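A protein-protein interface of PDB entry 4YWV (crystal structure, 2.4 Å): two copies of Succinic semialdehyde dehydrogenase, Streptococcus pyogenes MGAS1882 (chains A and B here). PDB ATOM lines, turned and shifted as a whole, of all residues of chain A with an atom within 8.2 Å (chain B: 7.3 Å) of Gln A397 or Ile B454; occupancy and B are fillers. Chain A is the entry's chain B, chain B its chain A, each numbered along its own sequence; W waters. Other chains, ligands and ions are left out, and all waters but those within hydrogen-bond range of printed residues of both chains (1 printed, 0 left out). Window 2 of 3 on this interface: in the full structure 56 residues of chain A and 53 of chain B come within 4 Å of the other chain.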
ATOM      1  N   ASP A 241      -3.966 -20.322  17.805  1.00  0.00           N
ATOM      2  CA  ASP A 241      -3.929 -18.876  18.024  1.00  0.00           C
ATOM      3  C   ASP A 241      -4.973 -18.398  19.031  1.00  0.00           C
ATOM      4  O   ASP A 241      -5.505 -17.294  18.923  1.00  0.00           O
ATOM      5  CB  ASP A 241      -4.115 -18.150  16.689  1.00  0.00           C
ATOM      6  CG  ASP A 241      -5.419 -18.506  16.004  1.00  0.00           C
ATOM      7  OD1 ASP A 241      -5.792 -19.700  15.992  1.00  0.00           O
ATOM      8  OD2 ASP A 241      -6.067 -17.594  15.460  1.00  0.00           O
ATOM      9  N   GLN A 246      -8.097 -14.475  27.560  1.00  0.00           N
ATOM     10  CA  GLN A 246      -9.547 -14.492  27.452  1.00  0.00           C
ATOM     11  C   GLN A 246     -10.033 -15.902  27.815  1.00  0.00           C
ATOM     12  O   GLN A 246     -11.078 -16.078  28.446  1.00  0.00           O
ATOM     13  CB  GLN A 246      -9.966 -14.120  26.029  1.00  0.00           C
ATOM     14  CG  GLN A 246     -11.467 -14.122  25.817  1.00  0.00           C
ATOM     15  CD  GLN A 246     -11.863 -13.644  24.428  1.00  0.00           C
ATOM     16  OE1 GLN A 246     -11.229 -14.005  23.432  1.00  0.00           O
ATOM     17  NE2 GLN A 246     -12.926 -12.842  24.353  1.00  0.00           N
ATOM     18  N   ILE A 392     -15.140 -23.112  19.901  1.00  0.00           N
ATOM     19  CA  ILE A 392     -13.940 -22.960  19.087  1.00  0.00           C
ATOM     20  C   ILE A 392     -13.233 -21.742  19.667  1.00  0.00           C
ATOM     21  O   ILE A 392     -13.813 -20.656  19.714  1.00  0.00           O
ATOM     22  CB  ILE A 392     -14.258 -22.672  17.602  1.00  0.00           C
ATOM     23  CG1 ILE A 392     -15.169 -23.755  17.034  1.00  0.00           C
ATOM     24  CG2 ILE A 392     -12.961 -22.640  16.803  1.00  0.00           C
ATOM     25  CD1 ILE A 392     -14.519 -25.115  16.996  1.00  0.00           C
ATOM     26  N   PHE A 393     -11.995 -21.926  20.119  1.00  0.00           N
ATOM     27  CA  PHE A 393     -11.213 -20.834  20.695  1.00  0.00           C
ATOM     28  C   PHE A 393     -10.054 -20.459  19.779  1.00  0.00           C
ATOM     29  O   PHE A 393      -9.123 -21.242  19.576  1.00  0.00           O
ATOM     30  CB  PHE A 393     -10.694 -21.231  22.079  1.00  0.00           C
ATOM     31  CG  PHE A 393     -10.989 -20.213  23.140  1.00  0.00           C
ATOM     32  CD1 PHE A 393     -10.188 -19.082  23.284  1.00  0.00           C
ATOM     33  CD2 PHE A 393     -12.118 -20.339  23.941  1.00  0.00           C
ATOM     34  CE1 PHE A 393     -10.512 -18.089  24.207  1.00  0.00           C
ATOM     35  CE2 PHE A 393     -12.451 -19.352  24.865  1.00  0.00           C
ATOM     36  CZ  PHE A 393     -11.647 -18.224  24.997  1.00  0.00           C
ATOM     37  N   SER A 394     -10.130 -19.252  19.223  1.00  0.00           N
ATOM     38  CA  SER A 394      -9.118 -18.744  18.305  1.00  0.00           C
ATOM     39  C   SER A 394      -9.235 -17.227  18.209  1.00  0.00           C
ATOM     40  O   SER A 394     -10.345 -16.689  18.172  1.00  0.00           O
ATOM     41  CB  SER A 394      -9.328 -19.364  16.919  1.00  0.00           C
ATOM     42  OG  SER A 394      -8.476 -18.793  15.940  1.00  0.00           O
ATOM     43  N   SER A 395      -8.100 -16.538  18.167  1.00  0.00           N
ATOM     44  CA  SER A 395      -8.112 -15.079  18.071  1.00  0.00           C
ATOM     45  C   SER A 395      -8.567 -14.607  16.699  1.00  0.00           C
ATOM     46  O   SER A 395      -9.006 -13.470  16.542  1.00  0.00           O
ATOM     47  CB  SER A 395      -6.730 -14.507  18.369  1.00  0.00           C
ATOM     48  OG  SER A 395      -6.435 -14.629  19.747  1.00  0.00           O
ATOM     49  N   ASN A 396      -8.449 -15.488  15.710  1.00  0.00           N
ATOM     50  CA  ASN A 396      -8.856 -15.203  14.340  1.00  0.00           C
ATOM     51  C   ASN A 396     -10.284 -15.731  14.209  1.00  0.00           C
ATOM     52  O   ASN A 396     -10.512 -16.942  14.089  1.00  0.00           O
ATOM     53  CB  ASN A 396      -7.933 -15.937  13.378  1.00  0.00           C
ATOM     54  CG  ASN A 396      -8.176 -15.564  11.940  1.00  0.00           C
ATOM     55  OD1 ASN A 396      -9.319 -15.389  11.515  1.00  0.00           O
ATOM     56  ND2 ASN A 396      -7.101 -15.461  11.170  1.00  0.00           N
ATOM     57  N   GLN A 397     -11.248 -14.821  14.238  1.00  0.00           N
ATOM     58  CA  GLN A 397     -12.644 -15.214  14.162  1.00  0.00           C
ATOM     59  C   GLN A 397     -13.008 -15.813  12.804  1.00  0.00           C
ATOM     60  O   GLN A 397     -13.874 -16.693  12.714  1.00  0.00           O
ATOM     61  CB  GLN A 397     -13.532 -14.016  14.507  1.00  0.00           C
ATOM     62  CG  GLN A 397     -13.121 -13.338  15.814  1.00  0.00           C
ATOM     63  CD  GLN A 397     -14.177 -12.391  16.358  1.00  0.00           C
ATOM     64  OE1 GLN A 397     -14.809 -11.644  15.603  1.00  0.00           O
ATOM     65  NE2 GLN A 397     -14.361 -12.407  17.682  1.00  0.00           N
ATOM     66  N   GLU A 398     -12.348 -15.350  11.749  1.00  0.00           N
ATOM     67  CA  GLU A 398     -12.619 -15.897  10.423  1.00  0.00           C
ATOM     68  C   GLU A 398     -12.207 -17.373  10.499  1.00  0.00           C
ATOM     69  O   GLU A 398     -12.901 -18.264  10.006  1.00  0.00           O
ATOM     70  CB  GLU A 398     -11.801 -15.156   9.360  1.00  0.00           C
ATOM     71  CG  GLU A 398     -12.165 -15.525   7.944  1.00  0.00           C
ATOM     72  CD  GLU A 398     -11.272 -14.859   6.914  1.00  0.00           C
ATOM     73  OE1 GLU A 398     -11.373 -13.628   6.718  1.00  0.00           O
ATOM     74  OE2 GLU A 398     -10.460 -15.579   6.299  1.00  0.00           O
ATOM     75  N   HIS A 399     -11.077 -17.618  11.149  1.00  0.00           N
ATOM     76  CA  HIS A 399     -10.570 -18.968  11.317  1.00  0.00           C
ATOM     77  C   HIS A 399     -11.495 -19.788  12.219  1.00  0.00           C
ATOM     78  O   HIS A 399     -11.800 -20.941  11.918  1.00  0.00           O
ATOM     79  CB  HIS A 399      -9.184 -18.934  11.947  1.00  0.00           C
ATOM     80  CG  HIS A 399      -8.544 -20.281  12.055  1.00  0.00           C
ATOM     81  ND1 HIS A 399      -7.654 -20.605  13.056  1.00  0.00           N
ATOM     82  CD2 HIS A 399      -8.649 -21.381  11.273  1.00  0.00           C
ATOM     83  CE1 HIS A 399      -7.236 -21.847  12.885  1.00  0.00           C
ATOM     84  NE2 HIS A 399      -7.826 -22.340  11.810  1.00  0.00           N
ATOM     85  N   ALA A 400     -11.927 -19.194  13.330  1.00  0.00           N
ATOM     86  CA  ALA A 400     -12.804 -19.887  14.271  1.00  0.00           C
ATOM     87  C   ALA A 400     -14.092 -20.373  13.616  1.00  0.00           C
ATOM     88  O   ALA A 400     -14.532 -21.491  13.869  1.00  0.00           O
ATOM     89  CB  ALA A 400     -13.126 -18.981  15.440  1.00  0.00           C
ATOM     90  N   LYS A 401     -14.678 -19.522  12.773  1.00  0.00           N
ATOM     91  CA  LYS A 401     -15.918 -19.820  12.044  1.00  0.00           C
ATOM     92  C   LYS A 401     -15.740 -20.960  11.029  1.00  0.00           C
ATOM     93  O   LYS A 401     -16.601 -21.832  10.889  1.00  0.00           O
ATOM     94  CB  LYS A 401     -16.409 -18.553  11.321  1.00  0.00           C
ATOM     95  CG  LYS A 401     -17.069 -17.540  12.254  1.00  0.00           C
ATOM     96  CD  LYS A 401     -16.952 -16.098  11.769  1.00  0.00           C
ATOM     97  CE  LYS A 401     -17.801 -15.820  10.544  1.00  0.00           C
ATOM     98  NZ  LYS A 401     -17.576 -14.426  10.038  1.00  0.00           N
ATOM     99  N   ALA A 402     -14.614 -20.941  10.328  1.00  0.00           N
ATOM    100  CA  ALA A 402     -14.316 -21.949   9.324  1.00  0.00           C
ATOM    101  C   ALA A 402     -14.264 -23.321   9.964  1.00  0.00           C
ATOM    102  O   ALA A 402     -14.864 -24.272   9.467  1.00  0.00           O
ATOM    103  CB  ALA A 402     -12.991 -21.635   8.646  1.00  0.00           C
ATOM    104  N   VAL A 403     -13.549 -23.428  11.072  1.00  0.00           N
ATOM    105  CA  VAL A 403     -13.445 -24.704  11.744  1.00  0.00           C
ATOM    106  C   VAL A 403     -14.800 -25.144  12.291  1.00  0.00           C
ATOM    107  O   VAL A 403     -15.180 -26.305  12.149  1.00  0.00           O
ATOM    108  CB  VAL A 403     -12.413 -24.640  12.878  1.00  0.00           C
ATOM    109  CG1 VAL A 403     -12.533 -25.884  13.766  1.00  0.00           C
ATOM    110  CG2 VAL A 403     -11.006 -24.541  12.286  1.00  0.00           C
ATOM    111  N   ALA A 404     -15.533 -24.209  12.893  1.00  0.00           N
ATOM    112  CA  ALA A 404     -16.846 -24.507  13.460  1.00  0.00           C
ATOM    113  C   ALA A 404     -17.751 -25.196  12.452  1.00  0.00           C
ATOM    114  O   ALA A 404     -18.384 -26.205  12.762  1.00  0.00           O
ATOM    115  CB  ALA A 404     -17.511 -23.225  13.952  1.00  0.00           C
ATOM    116  N   SER A 412     -22.246 -23.724  17.821  1.00  0.00           N
ATOM    117  CA  SER A 412     -20.810 -23.541  17.968  1.00  0.00           C
ATOM    118  C   SER A 412     -20.570 -22.166  18.555  1.00  0.00           C
ATOM    119  O   SER A 412     -20.884 -21.153  17.924  1.00  0.00           O
ATOM    120  CB  SER A 412     -20.101 -23.655  16.618  1.00  0.00           C
ATOM    121  OG  SER A 412     -20.102 -24.994  16.172  1.00  0.00           O
ATOM    122  N   PHE A 413     -20.016 -22.133  19.760  1.00  0.00           N
ATOM    123  CA  PHE A 413     -19.744 -20.872  20.423  1.00  0.00           C
ATOM    124  C   PHE A 413     -18.286 -20.476  20.245  1.00  0.00           C
ATOM    125  O   PHE A 413     -17.388 -21.245  20.559  1.00  0.00           O
ATOM    126  CB  PHE A 413     -20.101 -21.000  21.903  1.00  0.00           C
ATOM    127  CG  PHE A 413     -21.531 -21.411  22.136  1.00  0.00           C
ATOM    128  CD1 PHE A 413     -22.559 -20.476  22.058  1.00  0.00           C
ATOM    129  CD2 PHE A 413     -21.854 -22.742  22.384  1.00  0.00           C
ATOM    130  CE1 PHE A 413     -23.882 -20.857  22.221  1.00  0.00           C
ATOM    131  CE2 PHE A 413     -23.180 -23.131  22.549  1.00  0.00           C
ATOM    132  CZ  PHE A 413     -24.197 -22.183  22.467  1.00  0.00           C
ATOM    133  N   ILE A 414     -18.059 -19.269  19.743  1.00  0.00           N
ATOM    134  CA  ILE A 414     -16.705 -18.762  19.505  1.00  0.00           C
ATOM    135  C   ILE A 414     -16.072 -18.022  20.703  1.00  0.00           C
ATOM    136  O   ILE A 414     -16.655 -17.088  21.251  1.00  0.00           O
ATOM    137  CB  ILE A 414     -16.702 -17.795  18.285  1.00  0.00           C
ATOM    138  CG1 ILE A 414     -17.431 -18.438  17.103  1.00  0.00           C
ATOM    139  CG2 ILE A 414     -15.276 -17.447  17.903  1.00  0.00           C
ATOM    140  CD1 ILE A 414     -16.838 -19.754  16.673  1.00  0.00           C
ATOM    141  N   ASN A 415     -14.868 -18.430  21.091  1.00  0.00           N
ATOM    142  CA  ASN A 415     -14.148 -17.787  22.194  1.00  0.00           C
ATOM    143  C   ASN A 415     -14.982 -17.560  23.435  1.00  0.00           C
ATOM    144  O   ASN A 415     -14.820 -16.543  24.118  1.00  0.00           O
ATOM    145  CB  ASN A 415     -13.580 -16.438  21.754  1.00  0.00           C
ATOM    146  CG  ASN A 415     -12.546 -16.576  20.678  1.00  0.00           C
ATOM    147  OD1 ASN A 415     -11.703 -17.476  20.727  1.00  0.00           O
ATOM    148  ND2 ASN A 415     -12.591 -15.682  19.693  1.00  0.00           N
ATOM    149  N   SER A 416     -15.861 -18.509  23.730  1.00  0.00           N
ATOM    150  CA  SER A 416     -16.729 -18.398  24.885  1.00  0.00           C
ATOM    151  C   SER A 416     -17.448 -19.704  25.177  1.00  0.00           C
ATOM    152  O   SER A 416     -17.492 -20.602  24.337  1.00  0.00           O
ATOM    153  CB  SER A 416     -17.765 -17.287  24.658  1.00  0.00           C
ATOM    154  OG  SER A 416     -18.515 -17.491  23.468  1.00  0.00           O
ATOM    155  N   THR A 419     -24.120 -20.131  25.567  1.00  0.00           N
ATOM    156  CA  THR A 419     -24.938 -18.954  25.777  1.00  0.00           C
ATOM    157  C   THR A 419     -26.320 -19.282  25.260  1.00  0.00           C
ATOM    158  O   THR A 419     -26.461 -19.990  24.269  1.00  0.00           O
ATOM    159  CB  THR A 419     -24.430 -17.768  24.956  1.00  0.00           C
ATOM    160  OG1 THR A 419     -23.196 -17.294  25.504  1.00  0.00           O
ATOM    161  CG2 THR A 419     -25.449 -16.652  24.949  1.00  0.00           C
ATOM    162  N   LEU A 424     -31.596 -16.652  19.683  1.00  0.00           N
ATOM    163  CA  LEU A 424     -30.756 -17.744  19.170  1.00  0.00           C
ATOM    164  C   LEU A 424     -31.390 -19.139  19.217  1.00  0.00           C
ATOM    165  O   LEU A 424     -31.821 -19.595  20.274  1.00  0.00           O
ATOM    166  CB  LEU A 424     -29.424 -17.782  19.937  1.00  0.00           C
ATOM    167  CG  LEU A 424     -28.559 -16.518  19.889  1.00  0.00           C
ATOM    168  CD1 LEU A 424     -27.381 -16.644  20.842  1.00  0.00           C
ATOM    169  CD2 LEU A 424     -28.078 -16.290  18.471  1.00  0.00           C
ATOM    170  N   THR B 110     -29.197  -9.648  16.808  1.00  0.00           N
ATOM    171  CA  THR B 110     -28.914  -9.724  18.232  1.00  0.00           C
ATOM    172  C   THR B 110     -27.912  -8.637  18.540  1.00  0.00           C
ATOM    173  O   THR B 110     -27.034  -8.363  17.730  1.00  0.00           O
ATOM    174  CB  THR B 110     -28.293 -11.097  18.633  1.00  0.00           C
ATOM    175  OG1 THR B 110     -27.907 -11.065  20.015  1.00  0.00           O
ATOM    176  CG2 THR B 110     -27.056 -11.406  17.787  1.00  0.00           C
ATOM    177  N   SER B 112     -26.090  -8.803  21.279  1.00  0.00           N
ATOM    178  CA  SER B 112     -25.161  -9.443  22.199  1.00  0.00           C
ATOM    179  C   SER B 112     -23.853  -9.798  21.496  1.00  0.00           C
ATOM    180  O   SER B 112     -22.807  -9.941  22.135  1.00  0.00           O
ATOM    181  CB  SER B 112     -25.796 -10.702  22.787  1.00  0.00           C
ATOM    182  OG  SER B 112     -26.895 -10.363  23.621  1.00  0.00           O
ATOM    183  N   GLY B 113     -23.922  -9.925  20.175  1.00  0.00           N
ATOM    184  CA  GLY B 113     -22.751 -10.260  19.387  1.00  0.00           C
ATOM    185  C   GLY B 113     -23.158 -10.549  17.955  1.00  0.00           C
ATOM    186  O   GLY B 113     -24.171 -10.034  17.476  1.00  0.00           O
ATOM    187  N   GLN B 114     -22.375 -11.373  17.267  1.00  0.00           N
ATOM    188  CA  GLN B 114     -22.671 -11.736  15.888  1.00  0.00           C
ATOM    189  C   GLN B 114     -23.157 -13.173  15.861  1.00  0.00           C
ATOM    190  O   GLN B 114     -22.510 -14.067  16.403  1.00  0.00           O
ATOM    191  CB  GLN B 114     -21.419 -11.596  15.032  1.00  0.00           C
ATOM    192  CG  GLN B 114     -20.781 -10.227  15.139  1.00  0.00           C
ATOM    193  CD  GLN B 114     -19.412 -10.175  14.496  1.00  0.00           C
ATOM    194  OE1 GLN B 114     -18.674  -9.198  14.654  1.00  0.00           O
ATOM    195  NE2 GLN B 114     -19.063 -11.229  13.760  1.00  0.00           N
ATOM    196  N   ALA B 115     -24.298 -13.403  15.225  1.00  0.00           N
ATOM    197  CA  ALA B 115     -24.846 -14.745  15.161  1.00  0.00           C
ATOM    198  C   ALA B 115     -25.531 -15.063  13.837  1.00  0.00           C
ATOM    199  O   ALA B 115     -26.096 -14.188  13.179  1.00  0.00           O
ATOM    200  CB  ALA B 115     -25.819 -14.940  16.306  1.00  0.00           C
ATOM    201  N   TYR B 116     -25.474 -16.327  13.446  1.00  0.00           N
ATOM    202  CA  TYR B 116     -26.121 -16.773  12.220  1.00  0.00           C
ATOM    203  C   TYR B 116     -26.104 -18.281  12.279  1.00  0.00           C
ATOM    204  O   TYR B 116     -25.515 -18.851  13.187  1.00  0.00           O
ATOM    205  CB  TYR B 116     -25.347 -16.294  10.992  1.00  0.00           C
ATOM    206  CG  TYR B 116     -23.965 -16.885  10.874  1.00  0.00           C
ATOM    207  CD1 TYR B 116     -23.774 -18.172  10.380  1.00  0.00           C
ATOM    208  CD2 TYR B 116     -22.846 -16.166  11.294  1.00  0.00           C
ATOM    209  CE1 TYR B 116     -22.506 -18.731  10.312  1.00  0.00           C
ATOM    210  CE2 TYR B 116     -21.576 -16.715  11.230  1.00  0.00           C
ATOM    211  CZ  TYR B 116     -21.410 -17.997  10.740  1.00  0.00           C
ATOM    212  OH  TYR B 116     -20.149 -18.540  10.694  1.00  0.00           O
ATOM    213  N   ILE B 452     -23.857 -20.381  14.910  1.00  0.00           N
ATOM    214  CA  ILE B 452     -22.474 -19.955  15.100  1.00  0.00           C
ATOM    215  C   ILE B 452     -22.636 -18.650  15.867  1.00  0.00           C
ATOM    216  O   ILE B 452     -23.255 -17.710  15.375  1.00  0.00           O
ATOM    217  CB  ILE B 452     -21.751 -19.656  13.767  1.00  0.00           C
ATOM    218  CG1 ILE B 452     -21.744 -20.898  12.867  1.00  0.00           C
ATOM    219  CG2 ILE B 452     -20.337 -19.180  14.049  1.00  0.00           C
ATOM    220  CD1 ILE B 452     -21.085 -22.107  13.470  1.00  0.00           C
ATOM    221  N   TYR B 453     -22.090 -18.586  17.075  1.00  0.00           N
ATOM    222  CA  TYR B 453     -22.262 -17.393  17.874  1.00  0.00           C
ATOM    223  C   TYR B 453     -20.970 -16.772  18.387  1.00  0.00           C
ATOM    224  O   TYR B 453     -20.120 -17.458  18.955  1.00  0.00           O
ATOM    225  CB  TYR B 453     -23.196 -17.713  19.047  1.00  0.00           C
ATOM    226  CG  TYR B 453     -23.441 -16.546  19.964  1.00  0.00           C
ATOM    227  CD1 TYR B 453     -24.046 -15.387  19.490  1.00  0.00           C
ATOM    228  CD2 TYR B 453     -23.027 -16.581  21.295  1.00  0.00           C
ATOM    229  CE1 TYR B 453     -24.229 -14.284  20.312  1.00  0.00           C
ATOM    230  CE2 TYR B 453     -23.203 -15.485  22.132  1.00  0.00           C
ATOM    231  CZ  TYR B 453     -23.807 -14.335  21.632  1.00  0.00           C
ATOM    232  OH  TYR B 453     -23.991 -13.235  22.440  1.00  0.00           O
ATOM    233  N   ILE B 454     -20.828 -15.464  18.178  1.00  0.00           N
ATOM    234  CA  ILE B 454     -19.656 -14.743  18.657  1.00  0.00           C
ATOM    235  C   ILE B 454     -20.107 -13.561  19.514  1.00  0.00           C
ATOM    236  O   ILE B 454     -20.654 -12.583  19.004  1.00  0.00           O
ATOM    237  CB  ILE B 454     -18.790 -14.212  17.501  1.00  0.00           C
ATOM    238  CG1 ILE B 454     -18.439 -15.356  16.544  1.00  0.00           C
ATOM    239  CG2 ILE B 454     -17.523 -13.580  18.058  1.00  0.00           C
ATOM    240  CD1 ILE B 454     -17.576 -14.943  15.358  1.00  0.00           C
ATOM    241  N   PRO B 455     -19.884 -13.645  20.836  1.00  0.00           N
ATOM    242  CA  PRO B 455     -20.247 -12.611  21.812  1.00  0.00           C
ATOM    243  C   PRO B 455     -19.397 -11.360  21.633  1.00  0.00           C
ATOM    244  O   PRO B 455     -18.279 -11.434  21.134  1.00  0.00           O
ATOM    245  CB  PRO B 455     -19.951 -13.276  23.156  1.00  0.00           C
ATOM    246  CG  PRO B 455     -19.934 -14.750  22.849  1.00  0.00           C
ATOM    247  CD  PRO B 455     -19.271 -14.799  21.510  1.00  0.00           C
ATOM    248  N   ASN B 456     -19.923 -10.211  22.049  1.00  0.00           N
ATOM    249  CA  ASN B 456     -19.177  -8.962  21.944  1.00  0.00           C
ATOM    250  C   ASN B 456     -18.121  -8.883  23.044  1.00  0.00           C
ATOM    251  O   ASN B 456     -18.363  -9.511  24.100  1.00  0.00           O
ATOM    252  CB  ASN B 456     -20.118  -7.761  22.061  1.00  0.00           C
ATOM    253  CG  ASN B 456     -21.018  -7.603  20.850  1.00  0.00           C
ATOM    254  OD1 ASN B 456     -20.591  -7.828  19.711  1.00  0.00           O
ATOM    255  ND2 ASN B 456     -22.263  -7.190  21.085  1.00  0.00           N
HETATM  256  O   HOH W   1     -19.157 -20.889   9.649  1.00  0.00           O
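O of Ser A412 sits at hydrogen-bond distance from N of Tyr B453 (3.0 Å). The backbone carbonyl oxygen of Tyr B453 is in hydrogen-bond range of the backbone NH of Ile A414 (2.9 Å).
The backbone NH of Gln B114 lies within hydrogen-bond range of the backbone carbonyl oxygen of Ile B454. The backbone NH of Ile B452 is in hydrogen-bond range of the backbone carbonyl oxygen of Tyr B116. N of Ile A392 is in hydrogen-bond range of O of Phe A413 (3.0 Å). O of Ile A414 sits at hydrogen-bond distance from OG of Ser A416 (2.9 Å).
Among the printed residues, pairs that only touch across the chains: Ser A416 with Pro B455, Ile A414 with Ile B454, Gln A397 with Ile B454, Leu A424 with Ala B115, Ser A412 with Ile B452, Ile A414 with Pro B455, Lys A401 with Tyr B116, Phe A413 with Tyr B453, Ala A404 with Ile B452, Thr A419 with Tyr B453, Leu A424 with Tyr B453 and Lys A401 with Ile B454.
Gln A397 touches one residue of chain B. Ile B454 touches three residues of chain A. Printed residues of chain B within 4 Å of Ser A412: Ile B452 and Tyr B453. Of the printed residues of chain A, Ile B452 touches Ala A404 (3.8 Å) and Ser A412 (3.5 Å). Of the printed residues of chain A, Tyr B116 touches Lys A401 (3.6 Å). Printed residues of chain B within 4 Å of Lys A401: Tyr B116 (3.6 Å) and Ile B454 (3.8 Å). Of the printed residues of chain A, Ala B115 touches Leu A424. Phe A393 touches none of the printed residues of chain B. The nearest residue of chain B that does not touch Gln A397 is Gln B114 (4.7 Å).
Hydrophobic or aromatic side chains of chain A that line the printed part of chain B: Ala A404, Phe A413, Ile A414 and Leu A424. Among the printed residues, 14 pairs touch across the chains.
No position is printed for both chains. Of the 14 pairs that touch across the chains among the printed residues, none has its exchanged pair printed and touching as well.
Water W1 bridges OH of Tyr B116 (2.8 Å) and O of Lys A401 (3.0 Å).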
